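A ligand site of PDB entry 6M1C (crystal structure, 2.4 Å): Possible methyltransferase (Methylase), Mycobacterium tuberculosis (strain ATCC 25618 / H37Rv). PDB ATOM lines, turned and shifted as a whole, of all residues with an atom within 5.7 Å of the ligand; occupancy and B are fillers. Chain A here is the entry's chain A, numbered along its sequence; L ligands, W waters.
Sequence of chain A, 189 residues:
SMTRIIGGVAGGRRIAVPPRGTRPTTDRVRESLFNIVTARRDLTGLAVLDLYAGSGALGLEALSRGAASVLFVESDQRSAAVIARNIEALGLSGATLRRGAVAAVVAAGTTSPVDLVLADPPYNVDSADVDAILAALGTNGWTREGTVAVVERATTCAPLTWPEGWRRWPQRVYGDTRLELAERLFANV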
ATOM      1  N   VAL A  17      -8.919   3.855 -15.358  1.00  0.00           N
ATOM      2  CA  VAL A  17      -7.779   4.661 -14.919  1.00  0.00           C
ATOM      3  C   VAL A  17      -8.260   6.087 -14.615  1.00  0.00           C
ATOM      4  O   VAL A  17      -9.089   6.634 -15.359  1.00  0.00           O
ATOM      5  CB  VAL A  17      -6.662   4.655 -15.973  1.00  0.00           C
ATOM      6  CG1 VAL A  17      -5.429   5.376 -15.456  1.00  0.00           C
ATOM      7  CG2 VAL A  17      -6.292   3.217 -16.356  1.00  0.00           C
ATOM      8  N   PRO A  18      -7.789   6.707 -13.543  1.00  0.00           N
ATOM      9  CA  PRO A  18      -8.154   8.117 -13.247  1.00  0.00           C
ATOM     10  C   PRO A  18      -7.532   9.061 -14.261  1.00  0.00           C
ATOM     11  O   PRO A  18      -6.751   8.597 -15.100  1.00  0.00           O
ATOM     12  CB  PRO A  18      -7.582   8.331 -11.823  1.00  0.00           C
ATOM     13  CG  PRO A  18      -7.434   6.953 -11.263  1.00  0.00           C
ATOM     14  CD  PRO A  18      -7.039   6.095 -12.431  1.00  0.00           C
ATOM     15  N   ARG A  23      -0.990  10.149 -14.131  1.00  0.00           N
ATOM     16  CA  ARG A  23       0.140   9.755 -14.955  1.00  0.00           C
ATOM     17  C   ARG A  23       0.430   8.285 -14.675  1.00  0.00           C
ATOM     18  O   ARG A  23       1.185   7.962 -13.743  1.00  0.00           O
ATOM     19  N   PRO A  24      -0.168   7.366 -15.440  1.00  0.00           N
ATOM     20  CA  PRO A  24      -0.137   5.942 -15.062  1.00  0.00           C
ATOM     21  C   PRO A  24       0.879   5.110 -15.818  1.00  0.00           C
ATOM     22  O   PRO A  24       1.462   5.516 -16.825  1.00  0.00           O
ATOM     23  CB  PRO A  24      -1.569   5.472 -15.380  1.00  0.00           C
ATOM     24  CG  PRO A  24      -2.184   6.591 -16.257  1.00  0.00           C
ATOM     25  CD  PRO A  24      -1.108   7.598 -16.550  1.00  0.00           C
ATOM     26  N   THR A  25       1.047   3.883 -15.317  1.00  0.00           N
ATOM     27  CA  THR A  25       2.046   2.957 -15.837  1.00  0.00           C
ATOM     28  C   THR A  25       1.664   2.461 -17.227  1.00  0.00           C
ATOM     29  O   THR A  25       0.485   2.190 -17.503  1.00  0.00           O
ATOM     30  CB  THR A  25       2.182   1.786 -14.864  1.00  0.00           C
ATOM     31  OG1 THR A  25       2.299   2.289 -13.531  1.00  0.00           O
ATOM     32  CG2 THR A  25       3.386   0.956 -15.196  1.00  0.00           C
ATOM     33  N   ASP A  50       0.604  -1.993  -2.066  1.00  0.00           N
ATOM     34  CA  ASP A  50       0.600  -1.192  -3.299  1.00  0.00           C
ATOM     35  C   ASP A  50       0.522   0.289  -2.938  1.00  0.00           C
ATOM     36  O   ASP A  50      -0.559   0.806  -2.654  1.00  0.00           O
ATOM     37  CB  ASP A  50      -0.554  -1.589  -4.228  1.00  0.00           C
ATOM     38  CG  ASP A  50      -0.503  -0.884  -5.602  1.00  0.00           C
ATOM     39  OD1 ASP A  50      -1.230  -1.328  -6.536  1.00  0.00           O
ATOM     40  OD2 ASP A  50       0.282   0.092  -5.771  1.00  0.00           O
ATOM     41  N   LEU A  51       1.654   0.981  -3.011  1.00  0.00           N
ATOM     42  CA  LEU A  51       1.756   2.368  -2.586  1.00  0.00           C
ATOM     43  C   LEU A  51       1.507   3.314  -3.744  1.00  0.00           C
ATOM     44  O   LEU A  51       2.008   3.093  -4.851  1.00  0.00           O
ATOM     45  CB  LEU A  51       3.134   2.641  -1.989  1.00  0.00           C
ATOM     46  CG  LEU A  51       3.366   1.692  -0.803  1.00  0.00           C
ATOM     47  CD1 LEU A  51       4.769   1.882  -0.237  1.00  0.00           C
ATOM     48  CD2 LEU A  51       2.274   1.891   0.290  1.00  0.00           C
ATOM     49  N   TYR A  52       0.765   4.396  -3.476  1.00  0.00           N
ATOM     50  CA  TYR A  52       0.380   5.341  -4.511  1.00  0.00           C
ATOM     51  C   TYR A  52      -0.369   4.590  -5.605  1.00  0.00           C
ATOM     52  O   TYR A  52      -0.009   4.643  -6.782  1.00  0.00           O
ATOM     53  CB  TYR A  52       1.589   6.081  -5.104  1.00  0.00           C
ATOM     54  CG  TYR A  52       2.512   6.655  -4.070  1.00  0.00           C
ATOM     55  CD1 TYR A  52       2.256   7.887  -3.500  1.00  0.00           C
ATOM     56  CD2 TYR A  52       3.631   5.963  -3.665  1.00  0.00           C
ATOM     57  CE1 TYR A  52       3.088   8.423  -2.565  1.00  0.00           C
ATOM     58  CE2 TYR A  52       4.476   6.486  -2.709  1.00  0.00           C
ATOM     59  CZ  TYR A  52       4.201   7.719  -2.164  1.00  0.00           C
ATOM     60  OH  TYR A  52       5.022   8.270  -1.213  1.00  0.00           O
ATOM     61  N   ALA A  53      -1.417   3.877  -5.192  1.00  0.00           N
ATOM     62  CA  ALA A  53      -2.000   2.846  -6.046  1.00  0.00           C
ATOM     63  C   ALA A  53      -2.625   3.405  -7.317  1.00  0.00           C
ATOM     64  O   ALA A  53      -2.722   2.675  -8.315  1.00  0.00           O
ATOM     65  CB  ALA A  53      -3.026   2.040  -5.241  1.00  0.00           C
ATOM     66  N   GLY A  54      -3.038   4.666  -7.341  1.00  0.00           N
ATOM     67  CA  GLY A  54      -3.650   5.226  -8.543  1.00  0.00           C
ATOM     68  C   GLY A  54      -4.889   4.483  -8.994  1.00  0.00           C
ATOM     69  O   GLY A  54      -5.960   4.636  -8.407  1.00  0.00           O
ATOM     70  N   SER A  55      -4.772   3.687 -10.044  1.00  0.00           N
ATOM     71  CA  SER A  55      -5.895   2.884 -10.511  1.00  0.00           C
ATOM     72  C   SER A  55      -5.944   1.511  -9.862  1.00  0.00           C
ATOM     73  O   SER A  55      -6.918   0.788 -10.078  1.00  0.00           O
ATOM     74  CB  SER A  55      -5.838   2.702 -12.025  1.00  0.00           C
ATOM     75  OG  SER A  55      -4.803   1.800 -12.382  1.00  0.00           O
ATOM     76  N   GLY A  56      -4.929   1.141  -9.094  1.00  0.00           N
ATOM     77  CA  GLY A  56      -4.800  -0.202  -8.585  1.00  0.00           C
ATOM     78  C   GLY A  56      -4.288  -1.226  -9.572  1.00  0.00           C
ATOM     79  O   GLY A  56      -4.296  -2.418  -9.251  1.00  0.00           O
ATOM     80  N   ALA A  57      -3.830  -0.800 -10.754  1.00  0.00           N
ATOM     81  CA  ALA A  57      -3.441  -1.729 -11.812  1.00  0.00           C
ATOM     82  C   ALA A  57      -2.399  -2.738 -11.333  1.00  0.00           C
ATOM     83  O   ALA A  57      -2.507  -3.944 -11.621  1.00  0.00           O
ATOM     84  CB  ALA A  57      -2.922  -0.961 -13.025  1.00  0.00           C
ATOM     85  N   LEU A  58      -1.369  -2.282 -10.620  1.00  0.00           N
ATOM     86  CA  LEU A  58      -0.314  -3.204 -10.197  1.00  0.00           C
ATOM     87  C   LEU A  58      -0.847  -4.230  -9.197  1.00  0.00           C
ATOM     88  O   LEU A  58      -0.614  -5.433  -9.346  1.00  0.00           O
ATOM     89  CB  LEU A  58       0.859  -2.424  -9.588  1.00  0.00           C
ATOM     90  CG  LEU A  58       1.506  -1.399 -10.519  1.00  0.00           C
ATOM     91  CD1 LEU A  58       2.756  -0.806  -9.914  1.00  0.00           C
ATOM     92  CD2 LEU A  58       1.825  -2.049 -11.839  1.00  0.00           C
ATOM     93  N   VAL A  73      -2.845   1.645  -1.070  1.00  0.00           N
ATOM     94  CA  VAL A  73      -2.715   2.902  -0.338  1.00  0.00           C
ATOM     95  C   VAL A  73      -2.666   4.044  -1.341  1.00  0.00           C
ATOM     96  O   VAL A  73      -1.819   4.060  -2.239  1.00  0.00           O
ATOM     97  CB  VAL A  73      -1.483   2.902   0.585  1.00  0.00           C
ATOM     98  CG1 VAL A  73      -1.467   4.158   1.435  1.00  0.00           C
ATOM     99  CG2 VAL A  73      -1.482   1.683   1.470  1.00  0.00           C
ATOM    100  N   GLU A  74      -3.560   5.017  -1.150  1.00  0.00           N
ATOM    101  CA  GLU A  74      -3.837   6.055  -2.147  1.00  0.00           C
ATOM    102  C   GLU A  74      -4.551   7.205  -1.446  1.00  0.00           C
ATOM    103  O   GLU A  74      -5.582   7.003  -0.824  1.00  0.00           O
ATOM    104  CB  GLU A  74      -4.701   5.487  -3.271  1.00  0.00           C
ATOM    105  CG  GLU A  74      -5.310   6.530  -4.190  1.00  0.00           C
ATOM    106  CD  GLU A  74      -4.262   7.281  -5.006  1.00  0.00           C
ATOM    107  OE1 GLU A  74      -3.308   6.640  -5.517  1.00  0.00           O
ATOM    108  OE2 GLU A  74      -4.403   8.516  -5.131  1.00  0.00           O
ATOM    109  N   SER A  75      -3.997   8.416  -1.558  1.00  0.00           N
ATOM    110  CA  SER A  75      -4.519   9.579  -0.856  1.00  0.00           C
ATOM    111  C   SER A  75      -5.621  10.312  -1.623  1.00  0.00           C
ATOM    112  O   SER A  75      -6.442  10.980  -0.989  1.00  0.00           O
ATOM    113  CB  SER A  75      -3.397  10.566  -0.537  1.00  0.00           C
ATOM    114  OG  SER A  75      -2.874  11.139  -1.733  1.00  0.00           O
ATOM    115  N   ASP A  76      -5.673  10.216  -2.948  1.00  0.00           N
ATOM    116  CA  ASP A  76      -6.717  10.916  -3.697  1.00  0.00           C
ATOM    117  C   ASP A  76      -8.021  10.126  -3.664  1.00  0.00           C
ATOM    118  O   ASP A  76      -8.045   8.929  -3.942  1.00  0.00           O
ATOM    119  CB  ASP A  76      -6.267  11.144  -5.132  1.00  0.00           C
ATOM    120  CG  ASP A  76      -7.373  11.732  -5.990  1.00  0.00           C
ATOM    121  OD1 ASP A  76      -7.702  12.920  -5.798  1.00  0.00           O
ATOM    122  OD2 ASP A  76      -7.908  11.016  -6.854  1.00  0.00           O
ATOM    123  N   SER A  79      -9.306   8.753  -6.992  1.00  0.00           N
ATOM    124  CA  SER A  79      -8.481   7.604  -7.355  1.00  0.00           C
ATOM    125  C   SER A  79      -8.892   6.375  -6.550  1.00  0.00           C
ATOM    126  O   SER A  79      -9.024   5.282  -7.101  1.00  0.00           O
ATOM    127  CB  SER A  79      -7.002   7.913  -7.121  1.00  0.00           C
ATOM    128  OG  SER A  79      -6.562   8.934  -7.991  1.00  0.00           O
ATOM    129  N   GLY A 100      -5.377   7.440   2.400  1.00  0.00           N
ATOM    130  CA  GLY A 100      -4.544   8.183   3.323  1.00  0.00           C
ATOM    131  C   GLY A 100      -3.218   8.488   2.666  1.00  0.00           C
ATOM    132  O   GLY A 100      -2.944   8.066   1.537  1.00  0.00           O
ATOM    133  N   ALA A 101      -2.400   9.251   3.393  1.00  0.00           N
ATOM    134  CA  ALA A 101      -1.107   9.681   2.902  1.00  0.00           C
ATOM    135  C   ALA A 101      -0.098   8.548   3.041  1.00  0.00           C
ATOM    136  O   ALA A 101       0.132   8.050   4.152  1.00  0.00           O
ATOM    137  CB  ALA A 101      -0.636  10.920   3.675  1.00  0.00           C
ATOM    138  N   VAL A 102       0.490   8.126   1.913  1.00  0.00           N
ATOM    139  CA  VAL A 102       1.356   6.947   1.903  1.00  0.00           C
ATOM    140  C   VAL A 102       2.431   7.040   2.983  1.00  0.00           C
ATOM    141  O   VAL A 102       2.613   6.118   3.772  1.00  0.00           O
ATOM    142  CB  VAL A 102       1.974   6.745   0.508  1.00  0.00           C
ATOM    143  CG1 VAL A 102       3.212   5.868   0.608  1.00  0.00           C
ATOM    144  CG2 VAL A 102       1.001   6.037  -0.409  1.00  0.00           C
ATOM    145  N   ALA A 103       3.146   8.169   3.040  1.00  0.00           N
ATOM    146  CA  ALA A 103       4.201   8.267   4.041  1.00  0.00           C
ATOM    147  C   ALA A 103       3.643   8.270   5.462  1.00  0.00           C
ATOM    148  O   ALA A 103       4.302   7.771   6.391  1.00  0.00           O
ATOM    149  CB  ALA A 103       5.063   9.512   3.777  1.00  0.00           C
ATOM    150  N   ASP A 120       4.521   3.517  -6.971  1.00  0.00           N
ATOM    151  CA  ASP A 120       4.571   4.367  -8.159  1.00  0.00           C
ATOM    152  C   ASP A 120       4.424   5.828  -7.750  1.00  0.00           C
ATOM    153  O   ASP A 120       3.415   6.472  -8.064  1.00  0.00           O
ATOM    154  CB  ASP A 120       3.497   3.981  -9.170  1.00  0.00           C
ATOM    155  CG  ASP A 120       3.591   4.791 -10.459  1.00  0.00           C
ATOM    156  OD1 ASP A 120       4.650   5.413 -10.700  1.00  0.00           O
ATOM    157  OD2 ASP A 120       2.605   4.796 -11.220  1.00  0.00           O
ATOM    158  N   PRO A 121       5.429   6.389  -7.097  1.00  0.00           N
ATOM    159  CA  PRO A 121       5.276   7.741  -6.534  1.00  0.00           C
ATOM    160  C   PRO A 121       5.122   8.791  -7.621  1.00  0.00           C
ATOM    161  O   PRO A 121       5.899   8.809  -8.597  1.00  0.00           O
ATOM    162  CB  PRO A 121       6.589   7.943  -5.753  1.00  0.00           C
ATOM    163  CG  PRO A 121       7.109   6.586  -5.526  1.00  0.00           C
ATOM    164  CD  PRO A 121       6.714   5.792  -6.727  1.00  0.00           C
ATOM    165  N   PRO A 122       4.142   9.680  -7.476  1.00  0.00           N
ATOM    166  CA  PRO A 122       3.970  10.776  -8.445  1.00  0.00           C
ATOM    167  C   PRO A 122       5.186  11.703  -8.460  1.00  0.00           C
ATOM    168  O   PRO A 122       6.076  11.626  -7.608  1.00  0.00           O
ATOM    169  CB  PRO A 122       2.716  11.488  -7.949  1.00  0.00           C
ATOM    170  CG  PRO A 122       2.696  11.200  -6.461  1.00  0.00           C
ATOM    171  CD  PRO A 122       3.256   9.811  -6.308  1.00  0.00           C
ATOM    172  N   ASN A 124       5.596  14.894  -7.959  1.00  0.00           N
ATOM    173  CA  ASN A 124       5.774  15.887  -6.912  1.00  0.00           C
ATOM    174  C   ASN A 124       6.573  15.352  -5.735  1.00  0.00           C
ATOM    175  O   ASN A 124       7.126  16.143  -4.966  1.00  0.00           O
ATOM    176  CB  ASN A 124       4.419  16.387  -6.401  1.00  0.00           C
ATOM    177  CG  ASN A 124       3.502  15.261  -6.018  1.00  0.00           C
ATOM    178  OD1 ASN A 124       3.512  14.211  -6.659  1.00  0.00           O
ATOM    179  ND2 ASN A 124       2.704  15.445  -4.966  1.00  0.00           N
ATOM    180  N   VAL A 125       6.640  14.035  -5.588  1.00  0.00           N
ATOM    181  CA  VAL A 125       7.402  13.413  -4.508  1.00  0.00           C
ATOM    182  C   VAL A 125       8.879  13.388  -4.881  1.00  0.00           C
ATOM    183  O   VAL A 125       9.238  12.931  -5.972  1.00  0.00           O
ATOM    184  CB  VAL A 125       6.871  11.994  -4.230  1.00  0.00           C
ATOM    185  CG1 VAL A 125       7.805  11.261  -3.300  1.00  0.00           C
ATOM    186  CG2 VAL A 125       5.445  12.059  -3.646  1.00  0.00           C
HETATM  187  N1  LIG L   1       0.315   2.922 -10.175  1.00  0.00           N
HETATM  188  C1  LIG L   1      -0.789   3.751 -10.644  1.00  0.00           C
HETATM  189  C2  LIG L   1      -1.394   3.278 -11.984  1.00  0.00           C
HETATM  190  O1  LIG L   1      -2.661   3.185 -12.082  1.00  0.00           O
HETATM  191  O2  LIG L   1      -0.614   3.012 -12.990  1.00  0.00           O
HETATM  192  C3  LIG L   1      -0.354   5.236 -10.829  1.00  0.00           C
HETATM  193  C4  LIG L   1       0.176   5.862  -9.526  1.00  0.00           C
HETATM  194  C5  LIG L   1       0.291   7.422  -9.738  1.00  0.00           C
HETATM  195  N2  LIG L   1       1.321   7.761 -10.718  1.00  0.00           N
HETATM  196  C6  LIG L   1       0.569   8.078  -8.323  1.00  0.00           C
HETATM  197  C7  LIG L   1      -0.777   8.115  -7.486  1.00  0.00           C
HETATM  198  O3  LIG L   1      -0.508   8.347  -6.239  1.00  0.00           O
HETATM  199  C8  LIG L   1      -1.734   9.291  -7.922  1.00  0.00           C
HETATM  200  O4  LIG L   1      -2.991   8.722  -7.996  1.00  0.00           O
HETATM  201  C9  LIG L   1      -1.669  10.298  -6.777  1.00  0.00           C
HETATM  202  O5  LIG L   1      -3.029  10.976  -6.690  1.00  0.00           O
HETATM  203  C10 LIG L   1      -1.444   9.561  -5.718  1.00  0.00           C
HETATM  204  N3  LIG L   1      -0.726  10.233  -4.664  1.00  0.00           N
HETATM  205  C11 LIG L   1       0.009  11.400  -4.623  1.00  0.00           C
HETATM  206  N4  LIG L   1       0.514  11.562  -3.379  1.00  0.00           N
HETATM  207  C12 LIG L   1       0.085  10.510  -2.640  1.00  0.00           C
HETATM  208  C13 LIG L   1       0.293  10.196  -1.312  1.00  0.00           C
HETATM  209  N5  LIG L   1       1.046  10.841  -0.221  1.00  0.00           N
HETATM  210  N6  LIG L   1      -0.249   9.060  -0.810  1.00  0.00           N
HETATM  211  C14 LIG L   1      -1.011   8.223  -1.648  1.00  0.00           C
HETATM  212  N7  LIG L   1      -1.230   8.528  -2.937  1.00  0.00           N
HETATM  213  C15 LIG L   1      -0.675   9.694  -3.446  1.00  0.00           C
HETATM  214  O   HOH W   1       1.570   1.727  -7.712  1.00  0.00           O
HETATM  215  O   HOH W   2      -0.960   0.461  -9.095  1.00  0.00           O
HETATM  216  O   HOH W   3       0.339  10.826 -11.497  1.00  0.00           O
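Residues that only touch the ligand: Pro 24 (3.6 Å), Tyr 52 (3.0 Å), Ala 53 (3.2 Å), Gly 54 (3.6 Å), Asp 76 (3.6 Å), Ser 79 (3.6 Å), Gly 100 (3.7 Å), Ala 101 (3.9 Å) and Pro 122 (3.3 Å).
Hydrophobic or aromatic side chains that line the ligand: Pro 24, Tyr 52, Val 102 and Pro 122.
Of the 28 residues printed, 16 come within 4 Å of the ligand.
Water W2 lies within hydrogen-bond range of O of Ala 53, N1 of the ligand, OD1 of Asp 50 and N of Leu 58.
Water W3 bridges N of Arg 23 (3.0 Å) and N2 of the ligand (3.3 Å).
A nitrogen (N2) of the ligand lies within hydrogen-bond range of the backbone carbonyl oxygen (O) of Arg 23 (3.0 Å).
The backbone NH of Ser 75 sits close to a nitrogen (N7) of the ligand (3.1 Å).
OD2 of Asp 120 lies within salt-bridge range of N1 of the ligand, at 3.1 Å.
The side-chain hydroxyl (OG) of Ser 75 lies close to a nitrogen (N7) of the ligand, 3.3 Å away.
OE2 of Glu 74 lies close to O4 of the ligand.
N of Val 102 sits at hydrogen-bond distance from N6 of the ligand, at 3.0 Å.
An oxygen (O1) of the ligand sits at hydrogen-bond distance from the backbone NH (N) of Ser 55, 3.0 Å away.
The backbone NH (N) of Thr 25 is in hydrogen-bond range of an oxygen (O2) of the ligand (3.0 Å).
O2 of the ligand sits at hydrogen-bond distance from OG1 of Thr 25, at 3.0 Å.
The side-chain hydroxyl (OG) of Ser 55 lies within hydrogen-bond range of an oxygen (O1) of the ligand, at 2.6 Å.
O of Gly 100 lies close to N of Ser 75.
The backbone NH of Ala 53 is in hydrogen-bond range of the backbone carbonyl oxygen of Val 73 (3.0 Å).
The side-chain hydroxyl (OG) of Ser 55 sits at hydrogen-bond distance from the backbone NH (N) of Ala 57 (3.2 Å).
N of Asp 120 sits at hydrogen-bond distance from O of Leu 51, at 3.3 Å.
The side-chain carboxylate (OE1) of Glu 74 sits at hydrogen-bond distance from the backbone NH (N) of Gly 54 (2.7 Å).
The backbone carbonyl oxygen (O) of Val 73 is in hydrogen-bond range of the backbone NH (N) of Tyr 52, 2.9 Å away.
O of Glu 74 is in hydrogen-bond range of N of Gly 100, 3.3 Å away.
The backbone NH (N) of Asp 76 lies within hydrogen-bond range of the side-chain carboxylate (OE2) of Glu 74 (3.0 Å).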
